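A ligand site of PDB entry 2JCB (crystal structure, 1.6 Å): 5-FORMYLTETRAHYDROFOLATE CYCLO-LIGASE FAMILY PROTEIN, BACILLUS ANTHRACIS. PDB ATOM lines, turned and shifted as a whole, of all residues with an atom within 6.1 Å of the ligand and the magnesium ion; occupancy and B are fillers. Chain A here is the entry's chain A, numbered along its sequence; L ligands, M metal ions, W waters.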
ATOM      1  N   ARG A  10     -19.297   4.687   5.863  1.00  0.00           N
ATOM      2  CA  ARG A  10     -20.620   5.315   5.882  1.00  0.00           C
ATOM      3  C   ARG A  10     -21.174   5.573   7.286  1.00  0.00           C
ATOM      4  O   ARG A  10     -21.758   6.645   7.528  1.00  0.00           O
ATOM      5  CB  ARG A  10     -21.618   4.460   5.090  1.00  0.00           C
ATOM      6  CG  ARG A  10     -21.154   4.094   3.685  1.00  0.00           C
ATOM      7  CD  ARG A  10     -20.951   5.312   2.808  1.00  0.00           C
ATOM      8  NE  ARG A  10     -22.174   6.111   2.743  1.00  0.00           N
ATOM      9  CZ  ARG A  10     -22.247   7.363   2.281  1.00  0.00           C
ATOM     10  NH1 ARG A  10     -21.184   8.004   1.805  1.00  0.00           N
ATOM     11  NH2 ARG A  10     -23.425   7.973   2.303  1.00  0.00           N
ATOM     12  N   LYS A  13     -19.331   8.566   8.835  1.00  0.00           N
ATOM     13  CA  LYS A  13     -19.861   9.802   8.260  1.00  0.00           C
ATOM     14  C   LYS A  13     -21.178  10.236   8.897  1.00  0.00           C
ATOM     15  O   LYS A  13     -21.358  11.418   9.196  1.00  0.00           O
ATOM     16  CB  LYS A  13     -20.049   9.620   6.757  1.00  0.00           C
ATOM     17  CG  LYS A  13     -18.882  10.122   5.906  1.00  0.00           C
ATOM     18  CD  LYS A  13     -19.278  10.204   4.416  1.00  0.00           C
ATOM     19  CE  LYS A  13     -18.037  10.307   3.524  1.00  0.00           C
ATOM     20  NZ  LYS A  13     -18.345  10.801   2.171  1.00  0.00           N
ATOM     21  N   ARG A  17     -21.615  13.407  11.199  1.00  0.00           N
ATOM     22  CA  ARG A  17     -22.655  14.374  10.718  1.00  0.00           C
ATOM     23  C   ARG A  17     -23.658  14.610  11.869  1.00  0.00           C
ATOM     24  O   ARG A  17     -23.898  15.743  12.253  1.00  0.00           O
ATOM     25  CB  ARG A  17     -23.371  13.831   9.478  1.00  0.00           C
ATOM     26  CG  ARG A  17     -24.028  14.908   8.603  1.00  0.00           C
ATOM     27  CD  ARG A  17     -24.728  14.249   7.374  1.00  0.00           C
ATOM     28  NE  ARG A  17     -23.783  13.996   6.271  1.00  0.00           N
ATOM     29  CZ  ARG A  17     -23.628  12.860   5.587  1.00  0.00           C
ATOM     30  NH1 ARG A  17     -24.377  11.769   5.813  1.00  0.00           N
ATOM     31  NH2 ARG A  17     -22.717  12.840   4.618  1.00  0.00           N
ATOM     32  N   ARG A  91     -29.279  15.293  -8.873  1.00  0.00           N
ATOM     33  CA  ARG A  91     -28.301  15.760  -7.872  1.00  0.00           C
ATOM     34  C   ARG A  91     -27.396  16.871  -8.420  1.00  0.00           C
ATOM     35  O   ARG A  91     -26.212  16.967  -8.088  1.00  0.00           O
ATOM     36  CB  ARG A  91     -27.502  14.587  -7.278  1.00  0.00           C
ATOM     37  CG  ARG A  91     -27.910  14.294  -5.850  1.00  0.00           C
ATOM     38  CD  ARG A  91     -28.969  13.226  -5.824  1.00  0.00           C
ATOM     39  NE  ARG A  91     -29.377  12.872  -4.462  1.00  0.00           N
ATOM     40  CZ  ARG A  91     -28.625  12.198  -3.601  1.00  0.00           C
ATOM     41  NH1 ARG A  91     -27.389  11.795  -3.896  1.00  0.00           N
ATOM     42  NH2 ARG A  91     -29.125  11.914  -2.406  1.00  0.00           N
ATOM     43  N   ARG A 143     -14.122  17.486   3.741  1.00  0.00           N
ATOM     44  CA  ARG A 143     -15.456  18.016   3.993  1.00  0.00           C
ATOM     45  C   ARG A 143     -16.517  16.916   4.058  1.00  0.00           C
ATOM     46  O   ARG A 143     -16.527  15.993   3.239  1.00  0.00           O
ATOM     47  CB  ARG A 143     -15.816  19.096   2.955  1.00  0.00           C
ATOM     48  CG  ARG A 143     -17.253  19.487   3.019  1.00  0.00           C
ATOM     49  CD  ARG A 143     -17.576  20.551   1.959  1.00  0.00           C
ATOM     50  NE  ARG A 143     -19.007  20.671   1.886  1.00  0.00           N
ATOM     51  CZ  ARG A 143     -19.838  19.888   1.187  1.00  0.00           C
ATOM     52  NH1 ARG A 143     -21.137  20.125   1.300  1.00  0.00           N
ATOM     53  NH2 ARG A 143     -19.409  18.879   0.445  1.00  0.00           N
ATOM     54  N   ILE A 144     -17.297  16.949   5.127  1.00  0.00           N
ATOM     55  CA  ILE A 144     -18.567  16.216   5.204  1.00  0.00           C
ATOM     56  C   ILE A 144     -19.703  17.244   5.101  1.00  0.00           C
ATOM     57  O   ILE A 144     -19.717  18.240   5.835  1.00  0.00           O
ATOM     58  CB  ILE A 144     -18.718  15.431   6.544  1.00  0.00           C
ATOM     59  CG1 ILE A 144     -17.698  14.309   6.676  1.00  0.00           C
ATOM     60  CG2 ILE A 144     -20.142  14.773   6.595  1.00  0.00           C
ATOM     61  CD1 ILE A 144     -17.627  13.738   8.058  1.00  0.00           C
ATOM     62  N   GLY A 145     -20.644  16.988   4.187  1.00  0.00           N
ATOM     63  CA  GLY A 145     -21.824  17.838   4.061  1.00  0.00           C
ATOM     64  C   GLY A 145     -23.021  17.132   4.719  1.00  0.00           C
ATOM     65  O   GLY A 145     -22.874  16.389   5.698  1.00  0.00           O
ATOM     66  N   TYR A 146     -24.197  17.342   4.130  1.00  0.00           N
ATOM     67  CA  TYR A 146     -25.482  16.889   4.702  1.00  0.00           C
ATOM     68  C   TYR A 146     -25.971  15.557   4.209  1.00  0.00           C
ATOM     69  O   TYR A 146     -26.952  15.015   4.729  1.00  0.00           O
ATOM     70  CB  TYR A 146     -26.567  17.979   4.469  1.00  0.00           C
ATOM     71  CG  TYR A 146     -26.303  19.144   5.337  1.00  0.00           C
ATOM     72  CD1 TYR A 146     -26.665  19.148   6.679  1.00  0.00           C
ATOM     73  CD2 TYR A 146     -25.597  20.225   4.839  1.00  0.00           C
ATOM     74  CE1 TYR A 146     -26.364  20.233   7.483  1.00  0.00           C
ATOM     75  CE2 TYR A 146     -25.274  21.306   5.635  1.00  0.00           C
ATOM     76  CZ  TYR A 146     -25.664  21.298   6.947  1.00  0.00           C
ATOM     77  OH  TYR A 146     -25.324  22.400   7.691  1.00  0.00           O
ATOM     78  N   GLY A 147     -25.263  14.982   3.246  1.00  0.00           N
ATOM     79  CA  GLY A 147     -25.557  13.660   2.775  1.00  0.00           C
ATOM     80  C   GLY A 147     -26.005  13.531   1.333  1.00  0.00           C
ATOM     81  O   GLY A 147     -26.071  12.406   0.825  1.00  0.00           O
ATOM     82  N   GLY A 148     -26.333  14.657   0.700  1.00  0.00           N
ATOM     83  CA  GLY A 148     -26.802  14.640  -0.696  1.00  0.00           C
ATOM     84  C   GLY A 148     -25.708  14.489  -1.758  1.00  0.00           C
ATOM     85  O   GLY A 148     -25.973  14.045  -2.873  1.00  0.00           O
ATOM     86  N   GLY A 149     -24.490  14.897  -1.400  1.00  0.00           N
ATOM     87  CA  GLY A 149     -23.362  14.856  -2.304  1.00  0.00           C
ATOM     88  C   GLY A 149     -23.477  15.873  -3.412  1.00  0.00           C
ATOM     89  O   GLY A 149     -22.894  15.717  -4.468  1.00  0.00           O
ATOM     90  N   TYR A 150     -24.252  16.926  -3.188  1.00  0.00           N
ATOM     91  CA  TYR A 150     -24.384  17.984  -4.203  1.00  0.00           C
ATOM     92  C   TYR A 150     -23.072  18.713  -4.543  1.00  0.00           C
ATOM     93  O   TYR A 150     -22.727  18.892  -5.723  1.00  0.00           O
ATOM     94  CB  TYR A 150     -25.402  19.052  -3.770  1.00  0.00           C
ATOM     95  CG  TYR A 150     -26.837  18.608  -3.956  1.00  0.00           C
ATOM     96  CD1 TYR A 150     -27.456  18.689  -5.209  1.00  0.00           C
ATOM     97  CD2 TYR A 150     -27.579  18.172  -2.860  1.00  0.00           C
ATOM     98  CE1 TYR A 150     -28.777  18.350  -5.365  1.00  0.00           C
ATOM     99  CE2 TYR A 150     -28.903  17.776  -3.012  1.00  0.00           C
ATOM    100  CZ  TYR A 150     -29.506  17.896  -4.271  1.00  0.00           C
ATOM    101  OH  TYR A 150     -30.808  17.516  -4.434  1.00  0.00           O
ATOM    102  N   TYR A 151     -22.355  19.148  -3.521  1.00  0.00           N
ATOM    103  CA  TYR A 151     -21.103  19.872  -3.780  1.00  0.00           C
ATOM    104  C   TYR A 151     -20.012  18.961  -4.302  1.00  0.00           C
ATOM    105  O   TYR A 151     -19.234  19.381  -5.154  1.00  0.00           O
ATOM    106  CB  TYR A 151     -20.647  20.735  -2.593  1.00  0.00           C
ATOM    107  CG  TYR A 151     -21.440  22.036  -2.541  1.00  0.00           C
ATOM    108  CD1 TYR A 151     -22.730  22.079  -1.989  1.00  0.00           C
ATOM    109  CD2 TYR A 151     -20.957  23.205  -3.163  1.00  0.00           C
ATOM    110  CE1 TYR A 151     -23.473  23.306  -2.005  1.00  0.00           C
ATOM    111  CE2 TYR A 151     -21.672  24.424  -3.171  1.00  0.00           C
ATOM    112  CZ  TYR A 151     -22.939  24.443  -2.589  1.00  0.00           C
ATOM    113  OH  TYR A 151     -23.653  25.578  -2.575  1.00  0.00           O
ATOM    114  N   ASP A 152     -19.978  17.696  -3.830  1.00  0.00           N
ATOM    115  CA  ASP A 152     -19.029  16.751  -4.347  1.00  0.00           C
ATOM    116  C   ASP A 152     -19.159  16.651  -5.880  1.00  0.00           C
ATOM    117  O   ASP A 152     -18.151  16.617  -6.575  1.00  0.00           O
ATOM    118  CB  ASP A 152     -19.225  15.380  -3.691  1.00  0.00           C
ATOM    119  CG  ASP A 152     -18.588  15.313  -2.306  1.00  0.00           C
ATOM    120  OD1 ASP A 152     -17.710  16.158  -1.970  1.00  0.00           O
ATOM    121  OD2 ASP A 152     -18.955  14.415  -1.526  1.00  0.00           O
ATOM    122  N   ARG A 153     -20.403  16.653  -6.396  1.00  0.00           N
ATOM    123  CA  ARG A 153     -20.654  16.519  -7.826  1.00  0.00           C
ATOM    124  C   ARG A 153     -20.332  17.830  -8.535  1.00  0.00           C
ATOM    125  O   ARG A 153     -19.718  17.849  -9.588  1.00  0.00           O
ATOM    126  CB  ARG A 153     -22.109  16.115  -8.065  1.00  0.00           C
ATOM    127  CG  ARG A 153     -22.423  14.721  -7.609  1.00  0.00           C
ATOM    128  CD  ARG A 153     -23.897  14.443  -7.887  1.00  0.00           C
ATOM    129  NE  ARG A 153     -24.305  13.056  -7.725  1.00  0.00           N
ATOM    130  CZ  ARG A 153     -24.547  12.494  -6.544  1.00  0.00           C
ATOM    131  NH1 ARG A 153     -24.995  11.253  -6.497  1.00  0.00           N
ATOM    132  NH2 ARG A 153     -24.339  13.204  -5.423  1.00  0.00           N
ATOM    133  N   VAL A 156     -16.582  18.977  -9.122  1.00  0.00           N
ATOM    134  CA  VAL A 156     -15.867  18.310 -10.240  1.00  0.00           C
ATOM    135  C   VAL A 156     -15.625  19.298 -11.394  1.00  0.00           C
ATOM    136  O   VAL A 156     -14.526  19.343 -11.927  1.00  0.00           O
ATOM    137  CB  VAL A 156     -16.639  17.082 -10.754  1.00  0.00           C
ATOM    138  CG1 VAL A 156     -15.920  16.439 -11.993  1.00  0.00           C
ATOM    139  CG2 VAL A 156     -16.767  16.053  -9.652  1.00  0.00           C
ATOM    140  N   GLU A 178     -14.030   9.435   0.767  1.00  0.00           N
ATOM    141  CA  GLU A 178     -14.181   8.540  -0.357  1.00  0.00           C
ATOM    142  C   GLU A 178     -13.632   9.199  -1.619  1.00  0.00           C
ATOM    143  O   GLU A 178     -13.400  10.418  -1.640  1.00  0.00           O
ATOM    144  CB  GLU A 178     -15.658   8.198  -0.472  1.00  0.00           C
ATOM    145  CG  GLU A 178     -16.250   7.809   0.878  1.00  0.00           C
ATOM    146  CD  GLU A 178     -17.682   7.282   0.800  1.00  0.00           C
ATOM    147  OE1 GLU A 178     -17.891   6.185   0.254  1.00  0.00           O
ATOM    148  OE2 GLU A 178     -18.590   7.988   1.310  1.00  0.00           O
ATOM    149  N   PHE A 180     -14.826  10.125  -4.431  1.00  0.00           N
ATOM    150  CA  PHE A 180     -15.631  11.287  -4.870  1.00  0.00           C
ATOM    151  C   PHE A 180     -15.717  12.545  -3.946  1.00  0.00           C
ATOM    152  O   PHE A 180     -16.303  13.522  -4.326  1.00  0.00           O
ATOM    153  CB  PHE A 180     -17.056  10.797  -5.153  1.00  0.00           C
ATOM    154  CG  PHE A 180     -17.674  10.090  -3.969  1.00  0.00           C
ATOM    155  CD1 PHE A 180     -18.140  10.835  -2.860  1.00  0.00           C
ATOM    156  CD2 PHE A 180     -17.714   8.677  -3.943  1.00  0.00           C
ATOM    157  CE1 PHE A 180     -18.663  10.196  -1.752  1.00  0.00           C
ATOM    158  CE2 PHE A 180     -18.257   8.029  -2.835  1.00  0.00           C
ATOM    159  CZ  PHE A 180     -18.736   8.794  -1.749  1.00  0.00           C
ATOM    160  N   ASP A 181     -15.205  12.490  -2.720  1.00  0.00           N
ATOM    161  CA  ASP A 181     -15.248  13.626  -1.803  1.00  0.00           C
ATOM    162  C   ASP A 181     -14.304  14.722  -2.310  1.00  0.00           C
ATOM    163  O   ASP A 181     -13.121  14.446  -2.546  1.00  0.00           O
ATOM    164  CB  ASP A 181     -14.862  13.171  -0.401  1.00  0.00           C
ATOM    165  CG  ASP A 181     -16.002  12.451   0.309  1.00  0.00           C
ATOM    166  OD1 ASP A 181     -17.176  12.754   0.015  1.00  0.00           O
ATOM    167  OD2 ASP A 181     -15.763  11.557   1.125  1.00  0.00           O
ATOM    168  N   LYS A 182     -14.844  15.915  -2.512  1.00  0.00           N
ATOM    169  CA  LYS A 182     -14.065  17.084  -2.982  1.00  0.00           C
ATOM    170  C   LYS A 182     -13.654  17.938  -1.799  1.00  0.00           C
ATOM    171  O   LYS A 182     -14.423  18.148  -0.851  1.00  0.00           O
ATOM    172  CB  LYS A 182     -14.855  17.892  -3.991  1.00  0.00           C
ATOM    173  CG  LYS A 182     -15.182  17.092  -5.304  1.00  0.00           C
ATOM    174  CD  LYS A 182     -13.940  16.653  -6.077  1.00  0.00           C
ATOM    175  CE  LYS A 182     -13.482  17.740  -7.034  1.00  0.00           C
ATOM    176  NZ  LYS A 182     -12.296  17.296  -7.820  1.00  0.00           N
HETATM  177  P1  LIG L   1     -21.795  14.632   1.608  1.00  0.00           P
HETATM  178  O1  LIG L   1     -23.006  15.530   1.370  1.00  0.00           O
HETATM  179  O2  LIG L   1     -21.389  14.634   3.035  1.00  0.00           O
HETATM  180  O3  LIG L   1     -20.755  14.995   0.564  1.00  0.00           O
HETATM  181  P2  LIG L   1     -21.527  11.883   0.627  1.00  0.00           P
HETATM  182  O4  LIG L   1     -20.059  12.150   0.441  1.00  0.00           O
HETATM  183  O5  LIG L   1     -21.872  10.682   1.345  1.00  0.00           O
HETATM  184  O6  LIG L   1     -22.307  13.144   1.298  1.00  0.00           O
HETATM  185  O7  LIG L   1     -22.177  11.718  -0.840  1.00  0.00           O
HETATM  186  C1  LIG L   1     -23.545  11.263  -0.858  1.00  0.00           C
HETATM  187  C2  LIG L   1     -23.823  10.397  -2.070  1.00  0.00           C
HETATM  188  O8  LIG L   1     -23.435  11.136  -3.219  1.00  0.00           O
HETATM  189  C3  LIG L   1     -22.974   9.137  -2.015  1.00  0.00           C
HETATM  190  O9  LIG L   1     -23.857   8.043  -2.097  1.00  0.00           O
HETATM  191  C4  LIG L   1     -22.054   9.230  -3.209  1.00  0.00           C
HETATM  192  O10 LIG L   1     -22.027   8.045  -3.938  1.00  0.00           O
HETATM  193  C5  LIG L   1     -22.669  10.309  -4.092  1.00  0.00           C
HETATM  194  N1  LIG L   1     -21.679  11.099  -4.875  1.00  0.00           N
HETATM  195  C6  LIG L   1     -20.889  12.067  -4.394  1.00  0.00           C
HETATM  196  N2  LIG L   1     -20.141  12.604  -5.388  1.00  0.00           N
HETATM  197  C7  LIG L   1     -20.445  11.982  -6.534  1.00  0.00           C
HETATM  198  C8  LIG L   1     -20.020  12.101  -7.956  1.00  0.00           C
HETATM  199  N3  LIG L   1     -19.087  12.998  -8.341  1.00  0.00           N
HETATM  200  N4  LIG L   1     -20.627  11.322  -8.855  1.00  0.00           N
HETATM  201  C9  LIG L   1     -21.546  10.408  -8.496  1.00  0.00           C
HETATM  202  N5  LIG L   1     -21.993  10.265  -7.231  1.00  0.00           N
HETATM  203  C10 LIG L   1     -21.499  11.021  -6.212  1.00  0.00           C
HETATM  204 MG    MG M   1     -18.933  13.914   0.326  1.00  0.00          MG
HETATM  205  O   HOH W   1     -21.071  17.012  -1.162  1.00  0.00           O
HETATM  206  O   HOH W   2     -16.970  14.182  -6.789  1.00  0.00           O
HETATM  207  O   HOH W   3     -18.307  13.134 -11.162  1.00  0.00           O
HETATM  208  O   HOH W   4     -27.056  10.696  -1.225  1.00  0.00           O
HETATM  209  O   HOH W   5     -23.912   8.264  -7.519  1.00  0.00           O
HETATM  210  O   HOH W   6     -17.687  15.584   0.665  1.00  0.00           O
HETATM  211  O   HOH W   7     -18.792  13.597   2.578  1.00  0.00           O
HETATM  212  O   HOH W   8     -23.069  10.357   3.952  1.00  0.00           O
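An oxygen (O2) of the ligand sits at hydrogen-bond distance from the backbone NH (N) of Gly 145, 2.7 Å away.
An oxygen (O2) of the ligand lies within salt-bridge range of the guanidinium group (NH2) of Arg 17 (2.7 Å).
An oxygen (O5) of the ligand lies within salt-bridge range of the side-chain amino group (NZ) of Lys 13, at 3.6 Å.
The guanidinium group (NH1) of Arg 10 lies within salt-bridge range of an oxygen (O5) of the ligand (2.8 Å).
N of Gly 147 is in hydrogen-bond range of O1 of the ligand, 3.0 Å away.
The guanidinium group of Arg 153 is in hydrogen-bond range of an oxygen (O8) of the ligand.
O1 of the ligand lies within hydrogen-bond range of N of Gly 149 (3.2 Å).
The side-chain carboxylate of Asp 152 sits at hydrogen-bond distance from the backbone NH of Lys 182, 2.9 Å away.
OD2 of Asp 181 is in salt-bridge range of NZ of Lys 13 (2.9 Å).
The backbone NH (N) of Glu 178 lies within hydrogen-bond range of the side-chain carboxylate (OD2) of Asp 181 (2.8 Å).
NZ of Lys 13 lies within salt-bridge range of OE2 of Glu 178 (3.0 Å).
The guanidinium group (NH1) of Arg 10 lies within salt-bridge range of the side-chain carboxylate (OE2) of Glu 178 (2.6 Å).
NH2 of Arg 153 is in hydrogen-bond range of O of Gly 149, at 3.1 Å.
O of Gly 148 is in hydrogen-bond range of NH2 of Arg 153 (3.1 Å).
O of Gly 148 sits at hydrogen-bond distance from NH1 of Arg 91 (2.8 Å).
Residues that only touch the ligand: Phe 180 (3.3 Å), Gly 148 (3.5 Å), Tyr 146 (3.5 Å) and Ile 144 (3.7 Å).
Hydrophobic or aromatic side chains that line the ligand: Ile 144 and Phe 180.
Of the 20 residues printed, 13 come within 4 Å of the ligand.
NZ of Lys 13 touches the magnesium ion (3.7 Å).
OD2 of Asp 152 binds the magnesium ion (1.9 Å).
The magnesium ion is bound by an oxygen (O4) of the ligand (2.1 Å).
Water W6 binds the magnesium ion, 2.1 Å away.
OD1 of Asp 181 is bound to the magnesium ion.
An oxygen (O3) of the ligand is bound to the magnesium ion (2.1 Å).
Water W7 binds the magnesium ion (2.3 Å).
The magnesium ion has six donor atoms within binding distance.
Water W7 lies within hydrogen-bond range of O2 of the ligand, NZ of Lys 13 and O of Arg 143.
Water W6 lies within hydrogen-bond range of the side-chain carboxylate (OD1) of Asp 152 and the backbone carbonyl oxygen (O) of Arg 143.
Water W5 lies within hydrogen-bond range of a nitrogen (N5) of the ligand (2.8 Å) and the guanidinium group (NH1) of Arg 153 (3.3 Å).
Water W2 lies within hydrogen-bond range of O of Phe 180, O of Asp 152 and N3 of the ligand.
Water W8 lies within hydrogen-bond range of the guanidinium group (NH2) of Arg 17, an oxygen (O5) of the ligand and the guanidinium group (NH2) of Arg 10.
Water W4 bridges the guanidinium group of Arg 91 (2.7 Å) and the backbone carbonyl oxygen of Gly 147 (2.8 Å).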
